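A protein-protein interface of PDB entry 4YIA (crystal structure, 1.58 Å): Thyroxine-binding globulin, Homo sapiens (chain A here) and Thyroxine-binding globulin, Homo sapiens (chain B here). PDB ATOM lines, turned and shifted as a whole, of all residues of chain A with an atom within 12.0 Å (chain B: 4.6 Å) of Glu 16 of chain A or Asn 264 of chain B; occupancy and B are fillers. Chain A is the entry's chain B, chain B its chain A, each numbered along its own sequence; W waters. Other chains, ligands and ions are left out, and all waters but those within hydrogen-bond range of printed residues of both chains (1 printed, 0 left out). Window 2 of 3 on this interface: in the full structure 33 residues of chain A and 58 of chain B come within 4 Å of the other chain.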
ATOM      1  N   LEU A  12      18.391  21.921   4.813  1.00  0.00           N
ATOM      2  CA  LEU A  12      17.446  21.121   5.522  1.00  0.00           C
ATOM      3  C   LEU A  12      17.396  19.717   4.917  1.00  0.00           C
ATOM      4  O   LEU A  12      17.350  19.585   3.672  1.00  0.00           O
ATOM      5  CB  LEU A  12      16.092  21.731   5.365  1.00  0.00           C
ATOM      6  CG  LEU A  12      14.928  21.055   5.997  1.00  0.00           C
ATOM      7  CD1 LEU A  12      15.003  20.963   7.540  1.00  0.00           C
ATOM      8  CD2 LEU A  12      13.504  21.516   5.667  1.00  0.00           C
ATOM      9  N   LEU A  13      17.388  18.682   5.754  1.00  0.00           N
ATOM     10  CA  LEU A  13      17.155  17.308   5.320  1.00  0.00           C
ATOM     11  C   LEU A  13      16.007  16.746   6.156  1.00  0.00           C
ATOM     12  O   LEU A  13      15.903  17.037   7.346  1.00  0.00           O
ATOM     13  CB  LEU A  13      18.384  16.442   5.554  1.00  0.00           C
ATOM     14  CG  LEU A  13      19.667  16.850   4.832  1.00  0.00           C
ATOM     15  CD1 LEU A  13      20.472  17.825   5.649  1.00  0.00           C
ATOM     16  CD2 LEU A  13      20.387  15.525   4.624  1.00  0.00           C
ATOM     17  N   ILE A  14      15.097  16.039   5.500  1.00  0.00           N
ATOM     18  CA  ILE A  14      14.027  15.255   6.220  1.00  0.00           C
ATOM     19  C   ILE A  14      14.307  13.791   5.926  1.00  0.00           C
ATOM     20  O   ILE A  14      14.304  13.396   4.760  1.00  0.00           O
ATOM     21  CB  ILE A  14      12.652  15.656   5.755  1.00  0.00           C
ATOM     22  CG1 ILE A  14      12.363  17.127   6.062  1.00  0.00           C
ATOM     23  CG2 ILE A  14      11.560  14.819   6.368  1.00  0.00           C
ATOM     24  CD1 ILE A  14      11.063  17.700   5.531  1.00  0.00           C
ATOM     25  N   LEU A  15      14.623  13.067   6.982  1.00  0.00           N
ATOM     26  CA  LEU A  15      14.999  11.669   6.920  1.00  0.00           C
ATOM     27  C   LEU A  15      14.018  10.728   7.545  1.00  0.00           C
ATOM     28  O   LEU A  15      13.389  11.033   8.541  1.00  0.00           O
ATOM     29  CB  LEU A  15      16.356  11.472   7.593  1.00  0.00           C
ATOM     30  CG  LEU A  15      17.463  12.595   7.363  1.00  0.00           C
ATOM     31  CD1 LEU A  15      18.703  12.610   8.281  1.00  0.00           C
ATOM     32  CD2 LEU A  15      17.935  12.310   5.998  1.00  0.00           C
ATOM     33  N   GLU A  16      13.900   9.527   6.953  1.00  0.00           N
ATOM     34  CA  GLU A  16      13.051   8.441   7.436  1.00  0.00           C
ATOM     35  C   GLU A  16      13.965   7.376   8.040  1.00  0.00           C
ATOM     36  O   GLU A  16      14.989   7.003   7.496  1.00  0.00           O
ATOM     37  CB  GLU A  16      12.199   7.892   6.301  1.00  0.00           C
ATOM     38  CG  GLU A  16      11.069   6.994   6.756  1.00  0.00           C
ATOM     39  CD  GLU A  16      11.493   5.530   6.821  1.00  0.00           C
ATOM     40  OE1 GLU A  16      12.587   5.195   6.392  1.00  0.00           O
ATOM     41  OE2 GLU A  16      10.673   4.766   7.321  1.00  0.00           O
ATOM     42  N   ARG A  17      13.533   6.879   9.198  1.00  0.00           N
ATOM     43  CA  ARG A  17      14.419   6.000  10.025  1.00  0.00           C
ATOM     44  C   ARG A  17      14.508   4.590   9.534  1.00  0.00           C
ATOM     45  O   ARG A  17      15.602   4.025   9.514  1.00  0.00           O
ATOM     46  CB  ARG A  17      14.000   5.997  11.476  1.00  0.00           C
ATOM     47  CG  ARG A  17      14.265   7.288  12.206  1.00  0.00           C
ATOM     48  CD  ARG A  17      13.787   7.179  13.645  1.00  0.00           C
ATOM     49  NE  ARG A  17      13.815   8.469  14.372  1.00  0.00           N
ATOM     50  CZ  ARG A  17      14.874   9.033  14.920  1.00  0.00           C
ATOM     51  NH1 ARG A  17      16.039   8.500  14.867  1.00  0.00           N
ATOM     52  NH2 ARG A  17      14.736  10.172  15.553  1.00  0.00           N
ATOM     53  N   SER A  18      13.378   3.997   9.218  1.00  0.00           N
ATOM     54  CA  SER A  18      13.388   2.501   8.914  1.00  0.00           C
ATOM     55  C   SER A  18      14.236   2.148   7.683  1.00  0.00           C
ATOM     56  O   SER A  18      14.881   1.078   7.678  1.00  0.00           O
ATOM     57  CB  SER A  18      11.994   2.017   8.846  1.00  0.00           C
ATOM     58  OG  SER A  18      11.375   2.240   7.604  1.00  0.00           O
ATOM     59  N   THR A  19      14.333   3.057   6.703  1.00  0.00           N
ATOM     60  CA  THR A  19      15.093   2.842   5.516  1.00  0.00           C
ATOM     61  C   THR A  19      16.339   3.696   5.428  1.00  0.00           C
ATOM     62  O   THR A  19      17.085   3.604   4.468  1.00  0.00           O
ATOM     63  CB  THR A  19      14.245   3.045   4.296  1.00  0.00           C
ATOM     64  OG1 THR A  19      13.877   4.419   4.162  1.00  0.00           O
ATOM     65  CG2 THR A  19      12.930   2.248   4.414  1.00  0.00           C
ATOM     66  N   ARG A  20      16.510   4.584   6.381  1.00  0.00           N
ATOM     67  CA  ARG A  20      17.612   5.520   6.330  1.00  0.00           C
ATOM     68  C   ARG A  20      17.662   6.329   4.977  1.00  0.00           C
ATOM     69  O   ARG A  20      18.706   6.431   4.277  1.00  0.00           O
ATOM     70  CB  ARG A  20      18.964   4.908   6.722  1.00  0.00           C
ATOM     71  CG  ARG A  20      18.846   4.220   8.060  1.00  0.00           C
ATOM     72  CD  ARG A  20      20.204   3.729   8.579  1.00  0.00           C
ATOM     73  NE  ARG A  20      21.071   4.766   9.101  1.00  0.00           N
ATOM     74  CZ  ARG A  20      20.945   5.485  10.226  1.00  0.00           C
ATOM     75  NH1 ARG A  20      21.882   6.380  10.550  1.00  0.00           N
ATOM     76  NH2 ARG A  20      19.949   5.347  11.029  1.00  0.00           N
ATOM     77  N   SER A  21      16.534   6.879   4.609  1.00  0.00           N
ATOM     78  CA  SER A  21      16.274   7.577   3.356  1.00  0.00           C
ATOM     79  C   SER A  21      16.192   9.094   3.535  1.00  0.00           C
ATOM     80  O   SER A  21      15.578   9.540   4.504  1.00  0.00           O
ATOM     81  CB  SER A  21      14.956   7.115   2.743  1.00  0.00           C
ATOM     82  OG  SER A  21      15.145   5.836   2.175  1.00  0.00           O
ATOM     83  N   ILE A  22      16.717   9.849   2.578  1.00  0.00           N
ATOM     84  CA  ILE A  22      16.465  11.312   2.468  1.00  0.00           C
ATOM     85  C   ILE A  22      15.167  11.493   1.767  1.00  0.00           C
ATOM     86  O   ILE A  22      15.097  11.306   0.537  1.00  0.00           O
ATOM     87  CB  ILE A  22      17.604  12.078   1.792  1.00  0.00           C
ATOM     88  CG1 ILE A  22      18.904  11.746   2.447  1.00  0.00           C
ATOM     89  CG2 ILE A  22      17.325  13.559   1.819  1.00  0.00           C
ATOM     90  CD1 ILE A  22      20.095  12.379   1.823  1.00  0.00           C
ATOM     91  N   LEU A  23      14.094  11.804   2.466  1.00  0.00           N
ATOM     92  CA  LEU A  23      12.819  12.104   1.845  1.00  0.00           C
ATOM     93  C   LEU A  23      12.789  13.444   1.109  1.00  0.00           C
ATOM     94  O   LEU A  23      12.200  13.543   0.031  1.00  0.00           O
ATOM     95  CB  LEU A  23      11.703  12.082   2.853  1.00  0.00           C
ATOM     96  CG  LEU A  23      11.585  10.846   3.728  1.00  0.00           C
ATOM     97  CD1 LEU A  23      10.341  11.041   4.605  1.00  0.00           C
ATOM     98  CD2 LEU A  23      11.336   9.607   2.854  1.00  0.00           C
ATOM     99  N   PHE A  24      13.349  14.469   1.744  1.00  0.00           N
ATOM    100  CA  PHE A  24      13.435  15.812   1.176  1.00  0.00           C
ATOM    101  C   PHE A  24      14.788  16.416   1.495  1.00  0.00           C
ATOM    102  O   PHE A  24      15.311  16.166   2.570  1.00  0.00           O
ATOM    103  CB  PHE A  24      12.294  16.699   1.717  1.00  0.00           C
ATOM    104  CG  PHE A  24      10.889  16.192   1.419  1.00  0.00           C
ATOM    105  CD1 PHE A  24      10.241  16.537   0.232  1.00  0.00           C
ATOM    106  CD2 PHE A  24      10.284  15.375   2.305  1.00  0.00           C
ATOM    107  CE1 PHE A  24       8.951  16.065  -0.063  1.00  0.00           C
ATOM    108  CE2 PHE A  24       9.043  14.846   1.982  1.00  0.00           C
ATOM    109  CZ  PHE A  24       8.406  15.194   0.829  1.00  0.00           C
ATOM    110  N   LEU A  25      15.254  17.267   0.601  1.00  0.00           N
ATOM    111  CA  LEU A  25      16.527  17.979   0.746  1.00  0.00           C
ATOM    112  C   LEU A  25      16.324  19.367   0.195  1.00  0.00           C
ATOM    113  O   LEU A  25      15.687  19.584  -0.823  1.00  0.00           O
ATOM    114  CB  LEU A  25      17.586  17.271  -0.048  1.00  0.00           C
ATOM    115  CG  LEU A  25      18.978  17.867  -0.099  1.00  0.00           C
ATOM    116  CD1 LEU A  25      19.595  18.185   1.210  1.00  0.00           C
ATOM    117  CD2 LEU A  25      19.970  17.054  -0.922  1.00  0.00           C
ATOM    118  N   LEU B 119       8.489   2.365   3.245  1.00  0.00           N
ATOM    119  CA  LEU B 119       8.096   3.740   3.447  1.00  0.00           C
ATOM    120  C   LEU B 119       6.599   3.865   3.667  1.00  0.00           C
ATOM    121  O   LEU B 119       6.139   4.592   4.514  1.00  0.00           O
ATOM    122  CB  LEU B 119       8.501   4.635   2.302  1.00  0.00           C
ATOM    123  CG  LEU B 119       9.969   4.861   2.092  1.00  0.00           C
ATOM    124  CD1 LEU B 119      10.243   5.671   0.831  1.00  0.00           C
ATOM    125  CD2 LEU B 119      10.595   5.558   3.321  1.00  0.00           C
ATOM    126  N   LYS B 123       2.623   3.623  10.319  1.00  0.00           N
ATOM    127  CA  LYS B 123       3.274   3.897  11.590  1.00  0.00           C
ATOM    128  C   LYS B 123       2.452   4.943  12.293  1.00  0.00           C
ATOM    129  O   LYS B 123       2.073   5.948  11.708  1.00  0.00           O
ATOM    130  CB  LYS B 123       4.696   4.371  11.386  1.00  0.00           C
ATOM    131  CG  LYS B 123       5.548   3.382  10.591  1.00  0.00           C
ATOM    132  CD  LYS B 123       7.030   3.646  10.764  1.00  0.00           C
ATOM    133  CE  LYS B 123       7.873   2.570  10.093  1.00  0.00           C
ATOM    134  NZ  LYS B 123       7.604   2.453   8.633  1.00  0.00           N
ATOM    135  N   LEU B 126       2.655   9.149  12.008  1.00  0.00           N
ATOM    136  CA  LEU B 126       3.352   9.623  10.829  1.00  0.00           C
ATOM    137  C   LEU B 126       2.480   9.416   9.598  1.00  0.00           C
ATOM    138  O   LEU B 126       2.007   8.303   9.416  1.00  0.00           O
ATOM    139  CB  LEU B 126       4.602   8.821  10.618  1.00  0.00           C
ATOM    140  CG  LEU B 126       5.298   9.041   9.271  1.00  0.00           C
ATOM    141  CD1 LEU B 126       5.753  10.465   9.074  1.00  0.00           C
ATOM    142  CD2 LEU B 126       6.461   8.095   9.207  1.00  0.00           C
ATOM    143  N   LEU B 128       2.888   9.221   5.762  1.00  0.00           N
ATOM    144  CA  LEU B 128       3.901   9.087   4.736  1.00  0.00           C
ATOM    145  C   LEU B 128       3.376   8.161   3.631  1.00  0.00           C
ATOM    146  O   LEU B 128       3.118   6.977   3.886  1.00  0.00           O
ATOM    147  CB  LEU B 128       5.283   8.625   5.242  1.00  0.00           C
ATOM    148  CG  LEU B 128       6.424   8.415   4.237  1.00  0.00           C
ATOM    149  CD1 LEU B 128       6.680   9.669   3.389  1.00  0.00           C
ATOM    150  CD2 LEU B 128       7.662   8.013   4.956  1.00  0.00           C
ATOM    151  N   SER B 262       7.809  12.858  15.903  1.00  0.00           N
ATOM    152  CA  SER B 262       7.387  11.953  16.957  1.00  0.00           C
ATOM    153  C   SER B 262       7.592  10.506  16.701  1.00  0.00           C
ATOM    154  O   SER B 262       7.906   9.809  17.707  1.00  0.00           O
ATOM    155  CB  SER B 262       5.998  12.298  17.400  1.00  0.00           C
ATOM    156  OG  SER B 262       5.113  11.965  16.461  1.00  0.00           O
ATOM    157  N   LYS B 263       7.539  10.072  15.428  1.00  0.00           N
ATOM    158  CA  LYS B 263       7.770   8.685  15.025  1.00  0.00           C
ATOM    159  C   LYS B 263       8.462   8.538  13.691  1.00  0.00           C
ATOM    160  O   LYS B 263       8.013   9.166  12.679  1.00  0.00           O
ATOM    161  CB  LYS B 263       6.435   7.916  15.028  1.00  0.00           C
ATOM    162  CG  LYS B 263       5.854   7.620  16.422  1.00  0.00           C
ATOM    163  CD  LYS B 263       6.867   7.092  17.439  1.00  0.00           C
ATOM    164  CE  LYS B 263       6.188   6.728  18.750  1.00  0.00           C
ATOM    165  NZ  LYS B 263       7.146   6.161  19.739  1.00  0.00           N
ATOM    166  N   ASN B 264       9.562   7.764  13.698  1.00  0.00           N
ATOM    167  CA  ASN B 264      10.131   7.181  12.462  1.00  0.00           C
ATOM    168  C   ASN B 264      10.760   8.220  11.506  1.00  0.00           C
ATOM    169  O   ASN B 264      11.057   7.914  10.373  1.00  0.00           O
ATOM    170  CB  ASN B 264       9.127   6.330  11.646  1.00  0.00           C
ATOM    171  CG  ASN B 264       9.798   5.586  10.450  1.00  0.00           C
ATOM    172  OD1 ASN B 264      10.895   4.971  10.560  1.00  0.00           O
ATOM    173  ND2 ASN B 264       9.106   5.595   9.296  1.00  0.00           N
ATOM    174  N   ALA B 265      10.982   9.453  11.956  1.00  0.00           N
ATOM    175  CA  ALA B 265      11.489  10.499  11.050  1.00  0.00           C
ATOM    176  C   ALA B 265      12.221  11.593  11.863  1.00  0.00           C
ATOM    177  O   ALA B 265      11.962  11.759  13.066  1.00  0.00           O
ATOM    178  CB  ALA B 265      10.332  11.042  10.232  1.00  0.00           C
HETATM  179  O   HOH W   1      11.798  10.077  15.452  1.00  0.00           O
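O of Asn 264 of chain B lies within hydrogen-bond range of N of Arg 17 of chain A, 2.9 Å away. OD1 of Asn 264 of chain B is in hydrogen-bond range of N of Ser 18 of chain A (3.0 Å). ND2 of Asn 264 of chain B lies within hydrogen-bond range of OE2 of Glu 16 of chain A (2.7 Å).
The backbone carbonyl oxygen (O) of Ser 21 of chain A is in hydrogen-bond range of the backbone NH (N) of Glu 16 of chain A (3.0 Å). The side-chain carboxylate (OE2) of Glu 16 of chain A lies within hydrogen-bond range of the side-chain hydroxyl (OG) of Ser 18 of chain A. OE1 of Glu 16 of chain A is in hydrogen-bond range of OG1 of Thr 19 of chain A (2.7 Å). The side-chain hydroxyl of Thr 19 of chain A lies within hydrogen-bond range of the side-chain hydroxyl of Ser 21 of chain A (2.8 Å).
Ala 265 of chain B touches Leu 15 of chain A (CA to O, 3.2 Å). Leu 119 of chain B touches Glu 16 of chain A (CD2 to CD, 3.6 Å). CG of Glu 16 of chain A touches CD2 of Leu 128 of chain B, 3.99 Å away. Ala 265 of chain B touches Arg 17 of chain A. Lys 123 of chain B touches Ser 18 of chain A. Thr 19 of chain A touches Leu 119 of chain B.
Of the printed residues of chain B, Glu 16 of chain A touches Leu 119, Leu 128 and Asn 264. Asn 264 of chain B touches just these residues of chain A: Glu 16 (2.7 Å), Arg 17 (2.9 Å) and Ser 18 (3.0 Å). Lys 123 of chain B touches just one residue of chain A: Ser 18. Ala 265 of chain B touches just these residues of chain A: Leu 15 and Arg 17. Of the printed residues of chain B, Arg 17 of chain A touches Asn 264 (2.9 Å) and Ala 265 (3.9 Å). Printed residues of chain B within 4 Å of Ser 18 of chain A: Lys 123 and Asn 264. Of the printed residues of chain B, Leu 15 of chain A touches Ala 265 (3.2 Å). Leu 23 of chain A touches none of the printed residues of chain B. The nearest residue of chain A that does not touch Asn 264 of chain B is Leu 15 of chain A (4.3 Å). The nearest printed residue of chain B that does not touch Arg 17 of chain A is Lys 263 of chain B (5.4 Å).
Printed residues of chain A that touch a printed residue of chain B: Leu 15, Glu 16, Arg 17, Ser 18 and Thr 19. Along chain B the printed residues that touch a printed residue of chain A span positions 119 to 265. Among the printed residues, 9 pairs touch across the chains.
Water W1 lies within hydrogen-bond range of NE of Arg 17 of chain A and O of Ala 265 of chain B.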
